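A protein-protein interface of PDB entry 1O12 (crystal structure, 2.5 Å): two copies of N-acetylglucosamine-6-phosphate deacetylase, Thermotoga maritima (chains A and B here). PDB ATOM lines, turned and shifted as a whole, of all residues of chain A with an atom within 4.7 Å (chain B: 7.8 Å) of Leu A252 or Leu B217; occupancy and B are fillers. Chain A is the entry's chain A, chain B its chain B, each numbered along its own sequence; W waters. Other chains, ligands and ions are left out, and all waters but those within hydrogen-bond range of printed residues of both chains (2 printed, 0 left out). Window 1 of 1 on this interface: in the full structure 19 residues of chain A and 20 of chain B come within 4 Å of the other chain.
Leu A217 touches Leu B252, and with the chains exchanged Leu A252 touches Leu B217.
Val A256 touches its own counterpart, Val B256.
Of the 13 pairs that touch across the chains among the printed residues, 3 have their exchanged pair printed and touching as well.
Of the 22 printed residues of chain B, 8 touch a printed residue of chain A.
Of the 11 printed residues of chain A, 7 touch a printed residue of chain B.
Among the printed residues, 13 pairs touch across the chains.
Among the printed residues, no Asp or Glu carboxylate lies within 4 Å of a Lys or Arg side-chain nitrogen of the other chain.
NZ of Lys A255 lies close to O of Leu B230, 3.5 Å away.
Among the printed residues, merely in contact across the chains: Leu A217 with Leu B252 (3.9 Å), Glu A248 with Ile B222 (3.8 Å), Met A249 with Leu B217 (3.8 Å), Met A249 with His B218 (3.8 Å), Met A249 with His B219 (3.0 Å), Met A249 with Ile B222 (3.6 Å), Lys A251 with Leu B230 (3.98 Å), Leu A252 with Leu B217 (3.7 Å), Leu A252 with Leu B229 (3.8 Å), Leu A252 with Leu B230 (3.95 Å), Lys A255 with Leu B229 (3.3 Å) and Val A256 with Val B256 (3.5 Å).
Water W1 bridges N of Leu B217 and O of Leu A217.
Water W2 bridges O of Val B256 and O of Lys A255.
Of the printed residues of chain B, Leu A252 touches Leu B217, Leu B229 and Leu B230.
Leu B217 touches just these residues of chain A: Met A249 (3.8 Å) and Leu A252 (3.7 Å).
Of the printed residues of chain A, His B219 touches Met A249 (3.0 Å).
Of the printed residues of chain B, Leu A217 touches Leu B252.
Of the printed residues of chain B, Met A249 touches Leu B217, His B218, His B219 and Ile B222.
Of the printed residues of chain B, Lys A255 touches Leu B229 and Leu B230.
Of the printed residues of chain A, Leu B229 touches Leu A252 (3.8 Å) and Lys A255 (3.3 Å).
Pro A216 touches none of the printed residues of chain B.
The nearest printed residue of chain A that does not touch Val B256 is Lys A255 (4.3 Å).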
ATOM      1  N   PRO A 216      10.885  -7.063 -29.643  1.00  0.00           N
ATOM      2  CA  PRO A 216      11.168  -5.641 -29.459  1.00  0.00           C
ATOM      3  C   PRO A 216       9.899  -4.778 -29.477  1.00  0.00           C
ATOM      4  O   PRO A 216       8.781  -5.256 -29.742  1.00  0.00           O
ATOM      5  CB  PRO A 216      12.070  -5.318 -30.642  1.00  0.00           C
ATOM      6  CG  PRO A 216      12.826  -6.616 -30.847  1.00  0.00           C
ATOM      7  CD  PRO A 216      11.728  -7.641 -30.709  1.00  0.00           C
ATOM      8  N   LEU A 217      10.092  -3.494 -29.200  1.00  0.00           N
ATOM      9  CA  LEU A 217       9.011  -2.533 -29.208  1.00  0.00           C
ATOM     10  C   LEU A 217       8.807  -2.025 -30.645  1.00  0.00           C
ATOM     11  O   LEU A 217       9.720  -1.455 -31.267  1.00  0.00           O
ATOM     12  CB  LEU A 217       9.377  -1.382 -28.288  1.00  0.00           C
ATOM     13  CG  LEU A 217       8.407  -0.219 -28.198  1.00  0.00           C
ATOM     14  CD1 LEU A 217       7.419  -0.518 -27.127  1.00  0.00           C
ATOM     15  CD2 LEU A 217       9.172   1.065 -27.870  1.00  0.00           C
ATOM     16  N   GLU A 248      23.473   3.017 -21.946  1.00  0.00           N
ATOM     17  CA  GLU A 248      22.392   3.880 -22.420  1.00  0.00           C
ATOM     18  C   GLU A 248      20.993   3.260 -22.189  1.00  0.00           C
ATOM     19  O   GLU A 248      20.077   3.957 -21.770  1.00  0.00           O
ATOM     20  CB  GLU A 248      22.571   4.211 -23.899  1.00  0.00           C
ATOM     21  CG  GLU A 248      23.863   4.924 -24.199  1.00  0.00           C
ATOM     22  CD  GLU A 248      25.088   4.017 -23.999  1.00  0.00           C
ATOM     23  OE1 GLU A 248      25.066   2.864 -24.500  1.00  0.00           O
ATOM     24  OE2 GLU A 248      26.077   4.469 -23.355  1.00  0.00           O
ATOM     25  N   MET A 249      20.831   1.965 -22.461  1.00  0.00           N
ATOM     26  CA  MET A 249      19.549   1.291 -22.247  1.00  0.00           C
ATOM     27  C   MET A 249      19.112   1.382 -20.788  1.00  0.00           C
ATOM     28  O   MET A 249      17.965   1.747 -20.483  1.00  0.00           O
ATOM     29  CB  MET A 249      19.645  -0.187 -22.597  1.00  0.00           C
ATOM     30  CG  MET A 249      18.663  -0.648 -23.658  1.00  0.00           C
ATOM     31  SD  MET A 249      16.777  -0.115 -23.438  1.00  0.00           S
ATOM     32  CE  MET A 249      15.990  -1.533 -24.543  1.00  0.00           C
ATOM     33  N   VAL A 250      20.031   1.001 -19.902  1.00  0.00           N
ATOM     34  CA  VAL A 250      19.786   1.061 -18.477  1.00  0.00           C
ATOM     35  C   VAL A 250      19.348   2.480 -18.128  1.00  0.00           C
ATOM     36  O   VAL A 250      18.377   2.682 -17.387  1.00  0.00           O
ATOM     37  CB  VAL A 250      21.072   0.738 -17.651  1.00  0.00           C
ATOM     38  CG1 VAL A 250      20.794   0.940 -16.171  1.00  0.00           C
ATOM     39  CG2 VAL A 250      21.518  -0.685 -17.918  1.00  0.00           C
ATOM     40  N   LYS A 251      20.078   3.466 -18.639  1.00  0.00           N
ATOM     41  CA  LYS A 251      19.732   4.855 -18.370  1.00  0.00           C
ATOM     42  C   LYS A 251      18.317   5.163 -18.843  1.00  0.00           C
ATOM     43  O   LYS A 251      17.595   5.904 -18.190  1.00  0.00           O
ATOM     44  CB  LYS A 251      20.709   5.794 -19.048  1.00  0.00           C
ATOM     45  CG  LYS A 251      21.018   7.037 -18.233  1.00  0.00           C
ATOM     46  CD  LYS A 251      22.268   7.766 -18.780  1.00  0.00           C
ATOM     47  CE  LYS A 251      23.503   6.841 -18.782  1.00  0.00           C
ATOM     48  NZ  LYS A 251      24.750   7.474 -19.339  1.00  0.00           N
ATOM     49  N   LEU A 252      17.931   4.585 -19.977  1.00  0.00           N
ATOM     50  CA  LEU A 252      16.591   4.769 -20.531  1.00  0.00           C
ATOM     51  C   LEU A 252      15.531   4.073 -19.660  1.00  0.00           C
ATOM     52  O   LEU A 252      14.529   4.683 -19.277  1.00  0.00           O
ATOM     53  CB  LEU A 252      16.528   4.226 -21.964  1.00  0.00           C
ATOM     54  CG  LEU A 252      15.158   4.273 -22.662  1.00  0.00           C
ATOM     55  CD1 LEU A 252      14.525   5.688 -22.516  1.00  0.00           C
ATOM     56  CD2 LEU A 252      15.324   3.866 -24.136  1.00  0.00           C
ATOM     57  N   VAL A 253      15.743   2.809 -19.333  1.00  0.00           N
ATOM     58  CA  VAL A 253      14.767   2.116 -18.498  1.00  0.00           C
ATOM     59  C   VAL A 253      14.616   2.861 -17.166  1.00  0.00           C
ATOM     60  O   VAL A 253      13.500   3.038 -16.645  1.00  0.00           O
ATOM     61  CB  VAL A 253      15.165   0.666 -18.228  1.00  0.00           C
ATOM     62  CG1 VAL A 253      14.172   0.046 -17.268  1.00  0.00           C
ATOM     63  CG2 VAL A 253      15.202  -0.104 -19.525  1.00  0.00           C
ATOM     64  N   TYR A 254      15.733   3.326 -16.623  1.00  0.00           N
ATOM     65  CA  TYR A 254      15.666   4.054 -15.362  1.00  0.00           C
ATOM     66  C   TYR A 254      14.804   5.311 -15.534  1.00  0.00           C
ATOM     67  O   TYR A 254      13.902   5.578 -14.728  1.00  0.00           O
ATOM     68  CB  TYR A 254      17.061   4.418 -14.894  1.00  0.00           C
ATOM     69  CG  TYR A 254      17.072   5.411 -13.769  1.00  0.00           C
ATOM     70  CD1 TYR A 254      16.418   5.139 -12.561  1.00  0.00           C
ATOM     71  CD2 TYR A 254      17.764   6.623 -13.896  1.00  0.00           C
ATOM     72  CE1 TYR A 254      16.457   6.043 -11.508  1.00  0.00           C
ATOM     73  CE2 TYR A 254      17.811   7.530 -12.854  1.00  0.00           C
ATOM     74  CZ  TYR A 254      17.162   7.240 -11.661  1.00  0.00           C
ATOM     75  OH  TYR A 254      17.261   8.133 -10.614  1.00  0.00           O
ATOM     76  N   LYS A 255      15.059   6.055 -16.605  1.00  0.00           N
ATOM     77  CA  LYS A 255      14.300   7.258 -16.913  1.00  0.00           C
ATOM     78  C   LYS A 255      12.776   7.011 -16.974  1.00  0.00           C
ATOM     79  O   LYS A 255      11.987   7.788 -16.427  1.00  0.00           O
ATOM     80  CB  LYS A 255      14.780   7.817 -18.231  1.00  0.00           C
ATOM     81  CG  LYS A 255      14.063   9.067 -18.658  1.00  0.00           C
ATOM     82  CD  LYS A 255      14.514   9.459 -20.051  1.00  0.00           C
ATOM     83  CE  LYS A 255      13.878  10.762 -20.482  1.00  0.00           C
ATOM     84  NZ  LYS A 255      14.405  11.843 -19.628  1.00  0.00           N
ATOM     85  N   VAL A 256      12.373   5.923 -17.622  1.00  0.00           N
ATOM     86  CA  VAL A 256      10.962   5.577 -17.771  1.00  0.00           C
ATOM     87  C   VAL A 256      10.318   4.922 -16.554  1.00  0.00           C
ATOM     88  O   VAL A 256       9.221   5.292 -16.156  1.00  0.00           O
ATOM     89  CB  VAL A 256      10.763   4.602 -18.944  1.00  0.00           C
ATOM     90  CG1 VAL A 256       9.289   4.306 -19.128  1.00  0.00           C
ATOM     91  CG2 VAL A 256      11.392   5.177 -20.209  1.00  0.00           C
ATOM     92  N   PHE B 210       8.348  10.104 -35.401  1.00  0.00           N
ATOM     93  CA  PHE B 210       8.854   9.095 -34.477  1.00  0.00           C
ATOM     94  C   PHE B 210       7.736   8.105 -34.226  1.00  0.00           C
ATOM     95  O   PHE B 210       6.611   8.501 -33.941  1.00  0.00           O
ATOM     96  CB  PHE B 210       9.210   9.782 -33.169  1.00  0.00           C
ATOM     97  CG  PHE B 210       9.758   8.873 -32.119  1.00  0.00           C
ATOM     98  CD1 PHE B 210      11.136   8.710 -31.972  1.00  0.00           C
ATOM     99  CD2 PHE B 210       8.901   8.220 -31.228  1.00  0.00           C
ATOM    100  CE1 PHE B 210      11.653   7.913 -30.944  1.00  0.00           C
ATOM    101  CE2 PHE B 210       9.415   7.416 -30.190  1.00  0.00           C
ATOM    102  CZ  PHE B 210      10.789   7.263 -30.048  1.00  0.00           C
ATOM    103  N   PRO B 211       8.030   6.803 -34.307  1.00  0.00           N
ATOM    104  CA  PRO B 211       9.346   6.232 -34.618  1.00  0.00           C
ATOM    105  C   PRO B 211       9.339   5.515 -35.967  1.00  0.00           C
ATOM    106  O   PRO B 211      10.202   4.697 -36.240  1.00  0.00           O
ATOM    107  CB  PRO B 211       9.556   5.259 -33.475  1.00  0.00           C
ATOM    108  CG  PRO B 211       8.185   4.649 -33.375  1.00  0.00           C
ATOM    109  CD  PRO B 211       7.212   5.823 -33.568  1.00  0.00           C
ATOM    110  N   LEU B 214      12.578   4.411 -38.505  1.00  0.00           N
ATOM    111  CA  LEU B 214      13.770   4.343 -37.662  1.00  0.00           C
ATOM    112  C   LEU B 214      13.981   2.900 -37.248  1.00  0.00           C
ATOM    113  O   LEU B 214      13.030   2.137 -37.185  1.00  0.00           O
ATOM    114  CB  LEU B 214      13.598   5.198 -36.406  1.00  0.00           C
ATOM    115  CG  LEU B 214      13.310   6.688 -36.546  1.00  0.00           C
ATOM    116  CD1 LEU B 214      12.984   7.254 -35.189  1.00  0.00           C
ATOM    117  CD2 LEU B 214      14.494   7.394 -37.131  1.00  0.00           C
ATOM    118  N   LYS B 215      15.233   2.541 -36.977  1.00  0.00           N
ATOM    119  CA  LYS B 215      15.585   1.198 -36.537  1.00  0.00           C
ATOM    120  C   LYS B 215      14.935   1.027 -35.158  1.00  0.00           C
ATOM    121  O   LYS B 215      14.827   1.982 -34.400  1.00  0.00           O
ATOM    122  CB  LYS B 215      17.112   1.090 -36.437  1.00  0.00           C
ATOM    123  CG  LYS B 215      17.636  -0.206 -35.849  1.00  0.00           C
ATOM    124  CD  LYS B 215      17.373  -1.436 -36.742  1.00  0.00           C
ATOM    125  CE  LYS B 215      18.033  -1.333 -38.126  1.00  0.00           C
ATOM    126  NZ  LYS B 215      19.531  -1.358 -38.044  1.00  0.00           N
ATOM    127  N   PRO B 216      14.475  -0.180 -34.820  1.00  0.00           N
ATOM    128  CA  PRO B 216      13.846  -0.366 -33.502  1.00  0.00           C
ATOM    129  C   PRO B 216      14.822  -0.271 -32.327  1.00  0.00           C
ATOM    130  O   PRO B 216      16.043  -0.347 -32.486  1.00  0.00           O
ATOM    131  CB  PRO B 216      13.239  -1.774 -33.593  1.00  0.00           C
ATOM    132  CG  PRO B 216      13.015  -1.955 -35.071  1.00  0.00           C
ATOM    133  CD  PRO B 216      14.276  -1.366 -35.671  1.00  0.00           C
ATOM    134  N   LEU B 217      14.261  -0.125 -31.141  1.00  0.00           N
ATOM    135  CA  LEU B 217      15.054  -0.051 -29.921  1.00  0.00           C
ATOM    136  C   LEU B 217      15.629  -1.451 -29.648  1.00  0.00           C
ATOM    137  O   LEU B 217      14.887  -2.426 -29.621  1.00  0.00           O
ATOM    138  CB  LEU B 217      14.129   0.364 -28.773  1.00  0.00           C
ATOM    139  CG  LEU B 217      14.629   0.590 -27.358  1.00  0.00           C
ATOM    140  CD1 LEU B 217      15.422   1.893 -27.307  1.00  0.00           C
ATOM    141  CD2 LEU B 217      13.420   0.677 -26.414  1.00  0.00           C
ATOM    142  N   HIS B 218      16.938  -1.570 -29.478  1.00  0.00           N
ATOM    143  CA  HIS B 218      17.510  -2.876 -29.160  1.00  0.00           C
ATOM    144  C   HIS B 218      18.198  -2.832 -27.791  1.00  0.00           C
ATOM    145  O   HIS B 218      18.550  -1.748 -27.311  1.00  0.00           O
ATOM    146  CB  HIS B 218      18.469  -3.320 -30.264  1.00  0.00           C
ATOM    147  CG  HIS B 218      17.772  -3.691 -31.530  1.00  0.00           C
ATOM    148  ND1 HIS B 218      18.254  -3.348 -32.778  1.00  0.00           N
ATOM    149  CD2 HIS B 218      16.600  -4.335 -31.739  1.00  0.00           C
ATOM    150  CE1 HIS B 218      17.405  -3.763 -33.700  1.00  0.00           C
ATOM    151  NE2 HIS B 218      16.392  -4.363 -33.097  1.00  0.00           N
ATOM    152  N   HIS B 219      18.405  -3.994 -27.173  1.00  0.00           N
ATOM    153  CA  HIS B 219      18.996  -4.055 -25.822  1.00  0.00           C
ATOM    154  C   HIS B 219      20.342  -3.367 -25.602  1.00  0.00           C
ATOM    155  O   HIS B 219      20.595  -2.794 -24.538  1.00  0.00           O
ATOM    156  CB  HIS B 219      19.070  -5.516 -25.321  1.00  0.00           C
ATOM    157  CG  HIS B 219      20.048  -6.370 -26.061  1.00  0.00           C
ATOM    158  ND1 HIS B 219      21.346  -6.561 -25.631  1.00  0.00           N
ATOM    159  CD2 HIS B 219      19.926  -7.075 -27.210  1.00  0.00           C
ATOM    160  CE1 HIS B 219      21.980  -7.349 -26.481  1.00  0.00           C
ATOM    161  NE2 HIS B 219      21.142  -7.676 -27.447  1.00  0.00           N
ATOM    162  N   ARG B 220      21.196  -3.393 -26.610  1.00  0.00           N
ATOM    163  CA  ARG B 220      22.502  -2.789 -26.479  1.00  0.00           C
ATOM    164  C   ARG B 220      22.548  -1.492 -27.291  1.00  0.00           C
ATOM    165  O   ARG B 220      22.984  -0.450 -26.793  1.00  0.00           O
ATOM    166  CB  ARG B 220      23.528  -3.805 -26.969  1.00  0.00           C
ATOM    167  CG  ARG B 220      24.921  -3.675 -26.426  1.00  0.00           C
ATOM    168  CD  ARG B 220      25.613  -5.013 -26.630  1.00  0.00           C
ATOM    169  NE  ARG B 220      26.916  -5.089 -25.983  1.00  0.00           N
ATOM    170  CZ  ARG B 220      27.686  -6.173 -25.996  1.00  0.00           C
ATOM    171  NH1 ARG B 220      27.271  -7.277 -26.629  1.00  0.00           N
ATOM    172  NH2 ARG B 220      28.875  -6.154 -25.381  1.00  0.00           N
ATOM    173  N   GLU B 221      22.075  -1.556 -28.537  1.00  0.00           N
ATOM    174  CA  GLU B 221      22.048  -0.392 -29.423  1.00  0.00           C
ATOM    175  C   GLU B 221      20.684   0.240 -29.349  1.00  0.00           C
ATOM    176  O   GLU B 221      19.738  -0.286 -29.913  1.00  0.00           O
ATOM    177  CB  GLU B 221      22.299  -0.802 -30.876  1.00  0.00           C
ATOM    178  CG  GLU B 221      23.528  -0.161 -31.499  1.00  0.00           C
ATOM    179  CD  GLU B 221      23.507   1.342 -31.392  1.00  0.00           C
ATOM    180  OE1 GLU B 221      24.576   1.925 -31.142  1.00  0.00           O
ATOM    181  OE2 GLU B 221      22.428   1.938 -31.555  1.00  0.00           O
ATOM    182  N   ILE B 222      20.564   1.367 -28.668  1.00  0.00           N
ATOM    183  CA  ILE B 222      19.254   1.984 -28.565  1.00  0.00           C
ATOM    184  C   ILE B 222      18.882   2.845 -29.781  1.00  0.00           C
ATOM    185  O   ILE B 222      17.733   3.289 -29.913  1.00  0.00           O
ATOM    186  CB  ILE B 222      19.129   2.796 -27.251  1.00  0.00           C
ATOM    187  CG1 ILE B 222      20.072   3.987 -27.256  1.00  0.00           C
ATOM    188  CG2 ILE B 222      19.444   1.887 -26.042  1.00  0.00           C
ATOM    189  CD1 ILE B 222      19.689   5.014 -26.198  1.00  0.00           C
ATOM    190  N   GLY B 223      19.847   3.070 -30.673  1.00  0.00           N
ATOM    191  CA  GLY B 223      19.590   3.834 -31.870  1.00  0.00           C
ATOM    192  C   GLY B 223      18.897   5.166 -31.669  1.00  0.00           C
ATOM    193  O   GLY B 223      18.810   5.674 -30.536  1.00  0.00           O
ATOM    194  N   ILE B 224      18.411   5.737 -32.773  1.00  0.00           N
ATOM    195  CA  ILE B 224      17.727   7.019 -32.732  1.00  0.00           C
ATOM    196  C   ILE B 224      16.464   6.946 -31.890  1.00  0.00           C
ATOM    197  O   ILE B 224      16.095   7.901 -31.209  1.00  0.00           O
ATOM    198  CB  ILE B 224      17.351   7.510 -34.146  1.00  0.00           C
ATOM    199  CG1 ILE B 224      18.613   7.664 -34.982  1.00  0.00           C
ATOM    200  CG2 ILE B 224      16.635   8.859 -34.059  1.00  0.00           C
ATOM    201  CD1 ILE B 224      18.392   8.381 -36.288  1.00  0.00           C
ATOM    202  N   THR B 225      15.779   5.821 -31.955  1.00  0.00           N
ATOM    203  CA  THR B 225      14.578   5.664 -31.143  1.00  0.00           C
ATOM    204  C   THR B 225      14.975   5.873 -29.677  1.00  0.00           C
ATOM    205  O   THR B 225      14.327   6.610 -28.949  1.00  0.00           O
ATOM    206  CB  THR B 225      13.941   4.252 -31.323  1.00  0.00           C
ATOM    207  OG1 THR B 225      13.437   4.130 -32.655  1.00  0.00           O
ATOM    208  CG2 THR B 225      12.791   4.046 -30.369  1.00  0.00           C
ATOM    209  N   GLY B 226      16.067   5.245 -29.261  1.00  0.00           N
ATOM    210  CA  GLY B 226      16.491   5.369 -27.882  1.00  0.00           C
ATOM    211  C   GLY B 226      16.894   6.779 -27.546  1.00  0.00           C
ATOM    212  O   GLY B 226      16.566   7.300 -26.484  1.00  0.00           O
ATOM    213  N   ALA B 227      17.631   7.389 -28.467  1.00  0.00           N
ATOM    214  CA  ALA B 227      18.098   8.752 -28.308  1.00  0.00           C
ATOM    215  C   ALA B 227      16.920   9.678 -28.126  1.00  0.00           C
ATOM    216  O   ALA B 227      16.948  10.545 -27.277  1.00  0.00           O
ATOM    217  CB  ALA B 227      18.912   9.176 -29.536  1.00  0.00           C
ATOM    218  N   GLY B 228      15.876   9.480 -28.918  1.00  0.00           N
ATOM    219  CA  GLY B 228      14.703  10.333 -28.831  1.00  0.00           C
ATOM    220  C   GLY B 228      13.896  10.204 -27.552  1.00  0.00           C
ATOM    221  O   GLY B 228      13.220  11.162 -27.133  1.00  0.00           O
ATOM    222  N   LEU B 229      13.945   9.030 -26.927  1.00  0.00           N
ATOM    223  CA  LEU B 229      13.221   8.831 -25.681  1.00  0.00           C
ATOM    224  C   LEU B 229      14.047   9.341 -24.511  1.00  0.00           C
ATOM    225  O   LEU B 229      13.532  10.056 -23.655  1.00  0.00           O
ATOM    226  CB  LEU B 229      12.874   7.361 -25.492  1.00  0.00           C
ATOM    227  CG  LEU B 229      11.838   6.924 -26.530  1.00  0.00           C
ATOM    228  CD1 LEU B 229      11.547   5.428 -26.469  1.00  0.00           C
ATOM    229  CD2 LEU B 229      10.571   7.717 -26.267  1.00  0.00           C
ATOM    230  N   LEU B 230      15.341   9.012 -24.530  1.00  0.00           N
ATOM    231  CA  LEU B 230      16.299   9.375 -23.493  1.00  0.00           C
ATOM    232  C   LEU B 230      16.657  10.854 -23.324  1.00  0.00           C
ATOM    233  O   LEU B 230      16.707  11.347 -22.197  1.00  0.00           O
ATOM    234  CB  LEU B 230      17.579   8.575 -23.713  1.00  0.00           C
ATOM    235  CG  LEU B 230      18.749   8.717 -22.727  1.00  0.00           C
ATOM    236  CD1 LEU B 230      18.302   8.292 -21.295  1.00  0.00           C
ATOM    237  CD2 LEU B 230      19.913   7.836 -23.214  1.00  0.00           C
ATOM    238  N   LEU B 231      16.919  11.553 -24.433  1.00  0.00           N
ATOM    239  CA  LEU B 231      17.293  12.980 -24.416  1.00  0.00           C
ATOM    240  C   LEU B 231      16.101  13.880 -24.209  1.00  0.00           C
ATOM    241  O   LEU B 231      15.188  13.893 -25.003  1.00  0.00           O
ATOM    242  CB  LEU B 231      17.957  13.357 -25.722  1.00  0.00           C
ATOM    243  CG  LEU B 231      19.210  12.559 -26.051  1.00  0.00           C
ATOM    244  CD1 LEU B 231      19.720  13.045 -27.407  1.00  0.00           C
ATOM    245  CD2 LEU B 231      20.278  12.735 -24.973  1.00  0.00           C
ATOM    246  N   LEU B 252       2.707   5.799 -24.330  1.00  0.00           N
ATOM    247  CA  LEU B 252       4.064   5.537 -23.872  1.00  0.00           C
ATOM    248  C   LEU B 252       5.008   6.737 -24.065  1.00  0.00           C
ATOM    249  O   LEU B 252       5.720   7.156 -23.128  1.00  0.00           O
ATOM    250  CB  LEU B 252       4.628   4.325 -24.613  1.00  0.00           C
ATOM    251  CG  LEU B 252       6.048   3.873 -24.236  1.00  0.00           C
ATOM    252  CD1 LEU B 252       6.193   3.739 -22.725  1.00  0.00           C
ATOM    253  CD2 LEU B 252       6.317   2.514 -24.897  1.00  0.00           C
ATOM    254  N   VAL B 256       6.812   9.244 -21.373  1.00  0.00           N
ATOM    255  CA  VAL B 256       8.242   9.482 -21.325  1.00  0.00           C
ATOM    256  C   VAL B 256       8.703  10.876 -21.640  1.00  0.00           C
ATOM    257  O   VAL B 256       9.596  11.402 -20.986  1.00  0.00           O
ATOM    258  CB  VAL B 256       8.987   8.567 -22.292  1.00  0.00           C
ATOM    259  CG1 VAL B 256      10.424   9.080 -22.511  1.00  0.00           C
ATOM    260  CG2 VAL B 256       9.011   7.172 -21.743  1.00  0.00           C
HETATM  261  O   HOH W   1      11.584   0.768 -30.835  1.00  0.00           O
HETATM  262  O   HOH W   2      10.277  10.088 -18.249  1.00  0.00           O
